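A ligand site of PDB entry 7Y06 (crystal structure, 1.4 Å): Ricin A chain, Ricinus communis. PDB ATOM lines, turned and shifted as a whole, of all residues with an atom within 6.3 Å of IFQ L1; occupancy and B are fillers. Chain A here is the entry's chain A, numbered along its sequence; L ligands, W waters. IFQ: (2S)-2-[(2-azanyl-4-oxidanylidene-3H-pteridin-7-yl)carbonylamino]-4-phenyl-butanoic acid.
Water W2 lies within hydrogen-bond range of an oxygen (OXT) of IFQ L1 (2.7 Å), the backbone NH (N) of Asp 131 (2.9 Å) and the backbone NH (N) of Tyr 130 (3.4 Å). Water W3 lies within hydrogen-bond range of the side-chain carboxylate of Glu 184, the backbone carbonyl oxygen of Glu 215 and a nitrogen (N) of IFQ L1.
N of Tyr 87 lies within hydrogen-bond range of OD1 of Asn 85 (3.0 Å). OH of Tyr 87 is in hydrogen-bond range of OD1 of Asn 129, 2.7 Å away. O of Asn 85 sits at hydrogen-bond distance from NH2 of Arg 187 (2.8 Å). The side-chain hydroxyl (OH) of Tyr 87 sits close to the backbone NH (N) of Gly 128 (3.4 Å). The side-chain carboxylate (OE1) of Glu 184 is in salt-bridge range of the guanidinium group (NH1) of Arg 187 (3.1 Å). OH of Tyr 130 lies within hydrogen-bond range of OE2 of Glu 184, at 2.6 Å. N of Phe 100 lies within hydrogen-bond range of O of Val 89, at 3.0 Å. NH1 of Arg 141 lies within salt-bridge range of OE1 of Glu 215 (2.9 Å).
N of Tyr 130 lies within hydrogen-bond range of OAW of IFQ L1, 2.9 Å away. NH2 of Arg 141 lies within salt-bridge range of O of IFQ L1 (3.3 Å). OD1 of Asn 216 lies close to O of IFQ L1 (3.0 Å). ND2 of Asn 85 lies within hydrogen-bond range of O of IFQ L2, 2.9 Å away. O of Val 88 lies within hydrogen-bond range of N2 of IFQ L1 (2.9 Å). The backbone carbonyl oxygen (O) of Gly 128 sits at hydrogen-bond distance from a nitrogen (N2) of IFQ L1 (3.1 Å). The guanidinium group (NH2) of Arg 187 is in hydrogen-bond range of an oxygen (O4) of IFQ L1.
O of Ala 86 sits close to O4 of IFQ L1, at 3.4 Å. Tyr 87 touches IFQ L1. Phe 100 touches IFQ L1. CA of Asn 129 touches N8 of IFQ L1, 3.6 Å away. Ile 179 touches IFQ L1. Ser 183 touches IFQ L1. OE2 of Glu 184 touches C6 of IFQ L1, at 3.8 Å. Glu 215 touches IFQ L1 (O to CB, 3.7 Å). Trp 218 touches IFQ L1. Hydrophobic or aromatic side chains within 4 Å of IFQ L1: Tyr 87, Val 88, Phe 100, Tyr 130, Ile 179 and Trp 218. Within 4 Å of IFQ L1: Ala 86, Tyr 87, Val 88, Phe 100, Gly 128, Asn 129, Tyr 130, Arg 141, Ile 179, Ser 183, Glu 184, Arg 187, Glu 215, Asn 216 and Trp 218.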
ATOM      1  N   ASN A  85     -14.957   8.509  -3.526  1.00  0.00           N
ATOM      2  CA  ASN A  85     -15.267   9.233  -4.759  1.00  0.00           C
ATOM      3  C   ASN A  85     -14.070   9.492  -5.673  1.00  0.00           C
ATOM      4  O   ASN A  85     -14.230  10.125  -6.710  1.00  0.00           O
ATOM      5  CB  ASN A  85     -16.000  10.545  -4.436  1.00  0.00           C
ATOM      6  CG  ASN A  85     -15.248  11.386  -3.421  1.00  0.00           C
ATOM      7  OD1 ASN A  85     -14.060  11.177  -3.167  1.00  0.00           O
ATOM      8  ND2 ASN A  85     -15.932  12.360  -2.830  1.00  0.00           N
ATOM      9  N   ALA A  86     -12.895   8.979  -5.279  1.00  0.00           N
ATOM     10  CA  ALA A  86     -11.603   9.234  -5.970  1.00  0.00           C
ATOM     11  C   ALA A  86     -11.184  10.713  -5.993  1.00  0.00           C
ATOM     12  O   ALA A  86     -10.294  11.095  -6.748  1.00  0.00           O
ATOM     13  CB  ALA A  86     -11.580   8.610  -7.368  1.00  0.00           C
ATOM     14  N   TYR A  87     -11.807  11.537  -5.141  1.00  0.00           N
ATOM     15  CA  TYR A  87     -11.546  12.975  -5.095  1.00  0.00           C
ATOM     16  C   TYR A  87     -10.129  13.253  -4.604  1.00  0.00           C
ATOM     17  O   TYR A  87      -9.705  12.710  -3.580  1.00  0.00           O
ATOM     18  CB  TYR A  87     -12.559  13.655  -4.181  1.00  0.00           C
ATOM     19  CG  TYR A  87     -12.677  15.157  -4.341  1.00  0.00           C
ATOM     20  CD1 TYR A  87     -13.595  15.694  -5.247  1.00  0.00           C
ATOM     21  CD2 TYR A  87     -11.905  16.025  -3.573  1.00  0.00           C
ATOM     22  CE1 TYR A  87     -13.733  17.067  -5.384  1.00  0.00           C
ATOM     23  CE2 TYR A  87     -12.030  17.412  -3.709  1.00  0.00           C
ATOM     24  CZ  TYR A  87     -12.940  17.916  -4.614  1.00  0.00           C
ATOM     25  OH  TYR A  87     -13.079  19.276  -4.759  1.00  0.00           O
ATOM     26  N   VAL A  88      -9.399  14.089  -5.346  1.00  0.00           N
ATOM     27  CA  VAL A  88      -8.073  14.530  -4.946  1.00  0.00           C
ATOM     28  C   VAL A  88      -8.266  15.630  -3.890  1.00  0.00           C
ATOM     29  O   VAL A  88      -8.707  16.734  -4.219  1.00  0.00           O
ATOM     30  CB  VAL A  88      -7.233  15.038  -6.139  1.00  0.00           C
ATOM     31  CG1 VAL A  88      -5.846  15.476  -5.687  1.00  0.00           C
ATOM     32  CG2 VAL A  88      -7.117  13.967  -7.220  1.00  0.00           C
ATOM     33  N   VAL A  89      -7.958  15.304  -2.639  1.00  0.00           N
ATOM     34  CA  VAL A  89      -8.205  16.235  -1.519  1.00  0.00           C
ATOM     35  C   VAL A  89      -7.026  17.183  -1.246  1.00  0.00           C
ATOM     36  O   VAL A  89      -7.196  18.225  -0.608  1.00  0.00           O
ATOM     37  CB  VAL A  89      -8.606  15.512  -0.205  1.00  0.00           C
ATOM     38  CG1 VAL A  89      -9.895  14.720  -0.394  1.00  0.00           C
ATOM     39  CG2 VAL A  89      -7.492  14.619   0.338  1.00  0.00           C
ATOM     40  N   PHE A 100      -7.250  21.225  -0.460  1.00  0.00           N
ATOM     41  CA  PHE A 100      -8.362  22.057  -0.906  1.00  0.00           C
ATOM     42  C   PHE A 100      -9.299  22.376   0.257  1.00  0.00           C
ATOM     43  O   PHE A 100      -9.371  21.604   1.223  1.00  0.00           O
ATOM     44  CB  PHE A 100      -9.146  21.383  -2.038  1.00  0.00           C
ATOM     45  CG  PHE A 100      -8.330  21.160  -3.274  1.00  0.00           C
ATOM     46  CD1 PHE A 100      -7.850  22.238  -4.014  1.00  0.00           C
ATOM     47  CD2 PHE A 100      -8.062  19.860  -3.710  1.00  0.00           C
ATOM     48  CE1 PHE A 100      -7.089  22.030  -5.160  1.00  0.00           C
ATOM     49  CE2 PHE A 100      -7.307  19.644  -4.856  1.00  0.00           C
ATOM     50  CZ  PHE A 100      -6.826  20.722  -5.596  1.00  0.00           C
ATOM     51  N   GLY A 128     -11.751  22.420  -4.423  1.00  0.00           N
ATOM     52  CA  GLY A 128     -11.039  21.734  -5.507  1.00  0.00           C
ATOM     53  C   GLY A 128     -11.837  21.248  -6.698  1.00  0.00           C
ATOM     54  O   GLY A 128     -11.294  20.504  -7.509  1.00  0.00           O
ATOM     55  N   ASN A 129     -13.107  21.625  -6.810  1.00  0.00           N
ATOM     56  CA  ASN A 129     -13.930  21.250  -7.964  1.00  0.00           C
ATOM     57  C   ASN A 129     -13.452  21.944  -9.239  1.00  0.00           C
ATOM     58  O   ASN A 129     -12.822  23.009  -9.172  1.00  0.00           O
ATOM     59  CB  ASN A 129     -15.408  21.558  -7.726  1.00  0.00           C
ATOM     60  CG  ASN A 129     -16.067  20.616  -6.728  1.00  0.00           C
ATOM     61  OD1 ASN A 129     -15.413  19.821  -6.062  1.00  0.00           O
ATOM     62  ND2 ASN A 129     -17.391  20.720  -6.624  1.00  0.00           N
ATOM     63  N   TYR A 130     -13.762  21.352 -10.396  1.00  0.00           N
ATOM     64  CA  TYR A 130     -13.349  21.905 -11.692  1.00  0.00           C
ATOM     65  C   TYR A 130     -13.743  23.369 -11.881  1.00  0.00           C
ATOM     66  O   TYR A 130     -12.926  24.162 -12.323  1.00  0.00           O
ATOM     67  CB  TYR A 130     -13.888  21.101 -12.873  1.00  0.00           C
ATOM     68  CG  TYR A 130     -13.301  19.721 -13.056  1.00  0.00           C
ATOM     69  CD1 TYR A 130     -11.934  19.468 -12.887  1.00  0.00           C
ATOM     70  CD2 TYR A 130     -14.119  18.668 -13.457  1.00  0.00           C
ATOM     71  CE1 TYR A 130     -11.412  18.197 -13.076  1.00  0.00           C
ATOM     72  CE2 TYR A 130     -13.608  17.394 -13.654  1.00  0.00           C
ATOM     73  CZ  TYR A 130     -12.257  17.167 -13.456  1.00  0.00           C
ATOM     74  OH  TYR A 130     -11.763  15.907 -13.661  1.00  0.00           O
ATOM     75  N   ASP A 131     -14.985  23.715 -11.518  1.00  0.00           N
ATOM     76  CA  ASP A 131     -15.474  25.091 -11.728  1.00  0.00           C
ATOM     77  C   ASP A 131     -14.587  26.144 -11.055  1.00  0.00           C
ATOM     78  O   ASP A 131     -14.224  27.131 -11.689  1.00  0.00           O
ATOM     79  CB  ASP A 131     -16.972  25.249 -11.368  1.00  0.00           C
ATOM     80  CG  ASP A 131     -17.327  24.809  -9.938  1.00  0.00           C
ATOM     81  OD1 ASP A 131     -16.448  24.495  -9.106  1.00  0.00           O
ATOM     82  OD2 ASP A 131     -18.544  24.781  -9.648  1.00  0.00           O
ATOM     83  N   LEU A 133     -11.390  25.574  -9.995  1.00  0.00           N
ATOM     84  CA  LEU A 133     -10.039  25.437 -10.546  1.00  0.00           C
ATOM     85  C   LEU A 133      -9.892  26.080 -11.930  1.00  0.00           C
ATOM     86  O   LEU A 133      -8.856  26.687 -12.218  1.00  0.00           O
ATOM     87  CB  LEU A 133      -9.590  23.966 -10.567  1.00  0.00           C
ATOM     88  CG  LEU A 133      -9.334  23.268  -9.223  1.00  0.00           C
ATOM     89  CD1 LEU A 133      -8.911  21.837  -9.492  1.00  0.00           C
ATOM     90  CD2 LEU A 133      -8.279  23.979  -8.367  1.00  0.00           C
ATOM     91  N   ARG A 141     -11.470  23.227 -18.932  1.00  0.00           N
ATOM     92  CA  ARG A 141     -10.937  21.901 -19.250  1.00  0.00           C
ATOM     93  C   ARG A 141     -10.782  21.686 -20.758  1.00  0.00           C
ATOM     94  O   ARG A 141      -9.785  21.120 -21.195  1.00  0.00           O
ATOM     95  CB  ARG A 141     -11.830  20.807 -18.664  1.00  0.00           C
ATOM     96  CG  ARG A 141     -11.620  20.524 -17.190  1.00  0.00           C
ATOM     97  CD  ARG A 141     -12.718  19.625 -16.679  1.00  0.00           C
ATOM     98  NE  ARG A 141     -13.984  20.349 -16.504  1.00  0.00           N
ATOM     99  CZ  ARG A 141     -15.197  19.799 -16.555  1.00  0.00           C
ATOM    100  NH1 ARG A 141     -15.356  18.496 -16.776  1.00  0.00           N
ATOM    101  NH2 ARG A 141     -16.269  20.553 -16.370  1.00  0.00           N
ATOM    102  N   ILE A 179      -6.033  15.537 -11.926  1.00  0.00           N
ATOM    103  CA  ILE A 179      -7.354  15.001 -11.599  1.00  0.00           C
ATOM    104  C   ILE A 179      -7.892  14.156 -12.753  1.00  0.00           C
ATOM    105  O   ILE A 179      -8.398  13.057 -12.553  1.00  0.00           O
ATOM    106  CB  ILE A 179      -8.342  16.118 -11.202  1.00  0.00           C
ATOM    107  CG1 ILE A 179      -7.941  16.766  -9.876  1.00  0.00           C
ATOM    108  CG2 ILE A 179      -9.769  15.572 -11.114  1.00  0.00           C
ATOM    109  CD1 ILE A 179      -8.460  18.180  -9.689  1.00  0.00           C
ATOM    110  N   SER A 183      -7.836  10.459 -11.447  1.00  0.00           N
ATOM    111  CA  SER A 183      -9.180  10.183 -10.943  1.00  0.00           C
ATOM    112  C   SER A 183     -10.191   9.873 -12.033  1.00  0.00           C
ATOM    113  O   SER A 183     -10.925   8.886 -11.932  1.00  0.00           O
ATOM    114  CB  SER A 183      -9.677  11.317 -10.042  1.00  0.00           C
ATOM    115  OG  SER A 183      -8.773  11.481  -8.961  1.00  0.00           O
ATOM    116  N   GLU A 184     -10.238  10.689 -13.095  1.00  0.00           N
ATOM    117  CA  GLU A 184     -11.203  10.444 -14.174  1.00  0.00           C
ATOM    118  C   GLU A 184     -10.875   9.183 -14.945  1.00  0.00           C
ATOM    119  O   GLU A 184     -11.778   8.442 -15.341  1.00  0.00           O
ATOM    120  CB  GLU A 184     -11.347  11.627 -15.131  1.00  0.00           C
ATOM    121  CG  GLU A 184     -11.786  12.941 -14.483  1.00  0.00           C
ATOM    122  CD  GLU A 184     -13.205  12.978 -13.939  1.00  0.00           C
ATOM    123  OE1 GLU A 184     -13.892  11.938 -13.852  1.00  0.00           O
ATOM    124  OE2 GLU A 184     -13.630  14.085 -13.551  1.00  0.00           O
ATOM    125  N   ARG A 187     -12.103   6.356 -12.867  1.00  0.00           N
ATOM    126  CA  ARG A 187     -13.571   6.278 -12.923  1.00  0.00           C
ATOM    127  C   ARG A 187     -14.103   5.717 -14.252  1.00  0.00           C
ATOM    128  O   ARG A 187     -15.097   4.989 -14.270  1.00  0.00           O
ATOM    129  CB  ARG A 187     -14.201   7.653 -12.686  1.00  0.00           C
ATOM    130  CG  ARG A 187     -14.039   8.210 -11.282  1.00  0.00           C
ATOM    131  CD  ARG A 187     -14.394   9.692 -11.263  1.00  0.00           C
ATOM    132  NE  ARG A 187     -14.111  10.300  -9.979  1.00  0.00           N
ATOM    133  CZ  ARG A 187     -13.661  11.538  -9.795  1.00  0.00           C
ATOM    134  NH1 ARG A 187     -13.415  12.337 -10.837  1.00  0.00           N
ATOM    135  NH2 ARG A 187     -13.443  11.994  -8.568  1.00  0.00           N
ATOM    136  N   GLU A 215     -17.162  13.209 -17.649  1.00  0.00           N
ATOM    137  CA  GLU A 215     -16.734  13.811 -16.373  1.00  0.00           C
ATOM    138  C   GLU A 215     -17.892  14.511 -15.677  1.00  0.00           C
ATOM    139  O   GLU A 215     -18.172  14.249 -14.501  1.00  0.00           O
ATOM    140  CB  GLU A 215     -15.589  14.794 -16.582  1.00  0.00           C
ATOM    141  CG  GLU A 215     -14.307  14.145 -17.079  1.00  0.00           C
ATOM    142  CD  GLU A 215     -13.230  15.144 -17.426  1.00  0.00           C
ATOM    143  OE1 GLU A 215     -13.466  16.375 -17.366  1.00  0.00           O
ATOM    144  OE2 GLU A 215     -12.115  14.695 -17.784  1.00  0.00           O
ATOM    145  N   ASN A 216     -18.595  15.367 -16.407  1.00  0.00           N
ATOM    146  CA  ASN A 216     -19.717  16.126 -15.864  1.00  0.00           C
ATOM    147  C   ASN A 216     -20.873  15.254 -15.404  1.00  0.00           C
ATOM    148  O   ASN A 216     -21.628  15.647 -14.514  1.00  0.00           O
ATOM    149  CB  ASN A 216     -20.211  17.151 -16.877  1.00  0.00           C
ATOM    150  CG  ASN A 216     -19.191  18.248 -17.159  1.00  0.00           C
ATOM    151  OD1 ASN A 216     -18.240  18.447 -16.394  1.00  0.00           O
ATOM    152  ND2 ASN A 216     -19.392  18.972 -18.246  1.00  0.00           N
ATOM    153  N   SER A 217     -21.021  14.074 -16.011  1.00  0.00           N
ATOM    154  CA  SER A 217     -22.158  13.187 -15.771  1.00  0.00           C
ATOM    155  C   SER A 217     -21.890  12.018 -14.822  1.00  0.00           C
ATOM    156  O   SER A 217     -22.781  11.187 -14.646  1.00  0.00           O
ATOM    157  CB  SER A 217     -22.692  12.655 -17.107  1.00  0.00           C
ATOM    158  OG  SER A 217     -23.001  13.724 -17.997  1.00  0.00           O
ATOM    159  N   TRP A 218     -20.704  11.944 -14.224  1.00  0.00           N
ATOM    160  CA  TRP A 218     -20.344  10.759 -13.420  1.00  0.00           C
ATOM    161  C   TRP A 218     -21.329  10.459 -12.291  1.00  0.00           C
ATOM    162  O   TRP A 218     -21.755   9.322 -12.131  1.00  0.00           O
ATOM    163  CB  TRP A 218     -18.924  10.869 -12.862  1.00  0.00           C
ATOM    164  CG  TRP A 218     -18.449   9.642 -12.125  1.00  0.00           C
ATOM    165  CD1 TRP A 218     -18.392   8.355 -12.612  1.00  0.00           C
ATOM    166  CD2 TRP A 218     -17.950   9.582 -10.786  1.00  0.00           C
ATOM    167  NE1 TRP A 218     -17.889   7.512 -11.650  1.00  0.00           N
ATOM    168  CE2 TRP A 218     -17.618   8.232 -10.519  1.00  0.00           C
ATOM    169  CE3 TRP A 218     -17.761  10.539  -9.773  1.00  0.00           C
ATOM    170  CZ2 TRP A 218     -17.085   7.819  -9.288  1.00  0.00           C
ATOM    171  CZ3 TRP A 218     -17.245  10.128  -8.542  1.00  0.00           C
ATOM    172  CH2 TRP A 218     -16.906   8.775  -8.311  1.00  0.00           C
ATOM    173  N   GLY A 219     -21.689  11.499 -11.534  1.00  0.00           N
ATOM    174  CA  GLY A 219     -22.667  11.369 -10.450  1.00  0.00           C
ATOM    175  C   GLY A 219     -24.039  10.948 -10.958  1.00  0.00           C
ATOM    176  O   GLY A 219     -24.663  10.046 -10.389  1.00  0.00           O
HETATM  177  C2  IFQ L   1     -10.816  17.246  -7.304  1.00  0.00           C
HETATM  178  C4  IFQ L   1     -11.527  15.146  -8.247  1.00  0.00           C
HETATM  179  C6  IFQ L   1     -14.406  15.927 -10.376  1.00  0.00           C
HETATM  180  N1  IFQ L   1     -11.799  17.876  -7.976  1.00  0.00           N
HETATM  181  N3  IFQ L   1     -10.655  15.872  -7.435  1.00  0.00           N
HETATM  182  CAR IFQ L   1     -17.576  16.539  -8.331  1.00  0.00           C
HETATM  183  CAS IFQ L   1     -16.645  15.841  -7.558  1.00  0.00           C
HETATM  184  CAT IFQ L   1     -16.282  14.533  -7.911  1.00  0.00           C
HETATM  185  CAU IFQ L   1     -16.845  13.918  -9.031  1.00  0.00           C
HETATM  186  CAV IFQ L   1     -17.787  14.626  -9.805  1.00  0.00           C
HETATM  187  CAQ IFQ L   1     -18.157  15.927  -9.452  1.00  0.00           C
HETATM  188  CAP IFQ L   1     -19.185  16.727 -10.298  1.00  0.00           C
HETATM  189  CB  IFQ L   1     -18.878  16.699 -11.815  1.00  0.00           C
HETATM  190  CA  IFQ L   1     -17.664  17.561 -12.293  1.00  0.00           C
HETATM  191  C   IFQ L   1     -18.036  19.049 -12.522  1.00  0.00           C
HETATM  192  OXT IFQ L   1     -18.650  19.649 -11.606  1.00  0.00           O
HETATM  193  O   IFQ L   1     -17.714  19.535 -13.620  1.00  0.00           O
HETATM  194  N   IFQ L   1     -16.414  17.263 -11.528  1.00  0.00           N
HETATM  195  CAL IFQ L   1     -15.568  18.031 -10.809  1.00  0.00           C
HETATM  196  OAW IFQ L   1     -15.743  19.221 -10.528  1.00  0.00           O
HETATM  197  C7  IFQ L   1     -14.522  17.311 -10.200  1.00  0.00           C
HETATM  198  N8  IFQ L   1     -13.632  17.916  -9.398  1.00  0.00           N
HETATM  199  C8A IFQ L   1     -12.660  17.218  -8.764  1.00  0.00           C
HETATM  200  N2  IFQ L   1      -9.976  17.923  -6.531  1.00  0.00           N
HETATM  201  O4  IFQ L   1     -11.374  13.937  -8.345  1.00  0.00           O
HETATM  202  C4A IFQ L   1     -12.545  15.834  -8.926  1.00  0.00           C
HETATM  203  N5  IFQ L   1     -13.416  15.185  -9.728  1.00  0.00           N
HETATM  204  C2  IFQ L   2     -13.788  15.366  -0.357  1.00  0.00           C
HETATM  205  C4  IFQ L   2     -14.120  17.692  -0.958  1.00  0.00           C
HETATM  206  C6  IFQ L   2     -16.817  17.721  -3.496  1.00  0.00           C
HETATM  207  N1  IFQ L   2     -14.750  15.000  -1.227  1.00  0.00           N
HETATM  208  N3  IFQ L   2     -13.452  16.720  -0.211  1.00  0.00           N
HETATM  209  CAR IFQ L   2     -21.166  14.020  -8.393  1.00  0.00           C
HETATM  210  CAS IFQ L   2     -22.317  14.677  -8.873  1.00  0.00           C
HETATM  211  CAT IFQ L   2     -23.576  14.326  -8.368  1.00  0.00           C
HETATM  212  CAU IFQ L   2     -23.688  13.324  -7.389  1.00  0.00           C
HETATM  213  CAV IFQ L   2     -22.540  12.684  -6.908  1.00  0.00           C
HETATM  214  CAQ IFQ L   2     -21.277  13.030  -7.407  1.00  0.00           C
HETATM  215  CAP IFQ L   2     -20.037  12.293  -6.875  1.00  0.00           C
HETATM  216  CB  IFQ L   2     -19.006  13.221  -6.191  1.00  0.00           C
HETATM  217  CA  IFQ L   2     -19.451  13.735  -4.809  1.00  0.00           C
HETATM  218  C   IFQ L   2     -19.757  12.572  -3.858  1.00  0.00           C
HETATM  219  OXT IFQ L   2     -20.957  12.248  -3.711  1.00  0.00           O
HETATM  220  O   IFQ L   2     -18.791  12.016  -3.291  1.00  0.00           O
HETATM  221  N   IFQ L   2     -18.382  14.543  -4.191  1.00  0.00           N
HETATM  222  CAL IFQ L   2     -18.099  15.848  -4.417  1.00  0.00           C
HETATM  223  OAW IFQ L   2     -18.768  16.581  -5.142  1.00  0.00           O
HETATM  224  C7  IFQ L   2     -17.087  16.347  -3.591  1.00  0.00           C
HETATM  225  N8  IFQ L   2     -16.380  15.497  -2.803  1.00  0.00           N
HETATM  226  C8A IFQ L   2     -15.423  15.922  -1.961  1.00  0.00           C
HETATM  227  N2  IFQ L   2     -13.154  14.452   0.354  1.00  0.00           N
HETATM  228  O4  IFQ L   2     -13.808  18.867  -0.803  1.00  0.00           O
HETATM  229  C4A IFQ L   2     -15.120  17.281  -1.858  1.00  0.00           C
HETATM  230  N5  IFQ L   2     -15.801  18.172  -2.608  1.00  0.00           N
HETATM  231  O   HOH W   1     -18.831  22.274 -13.267  1.00  0.00           O
HETATM  232  O   HOH W   2     -17.087  21.744 -10.900  1.00  0.00           O
HETATM  233  O   HOH W   3     -16.132  14.748 -12.749  1.00  0.00           O
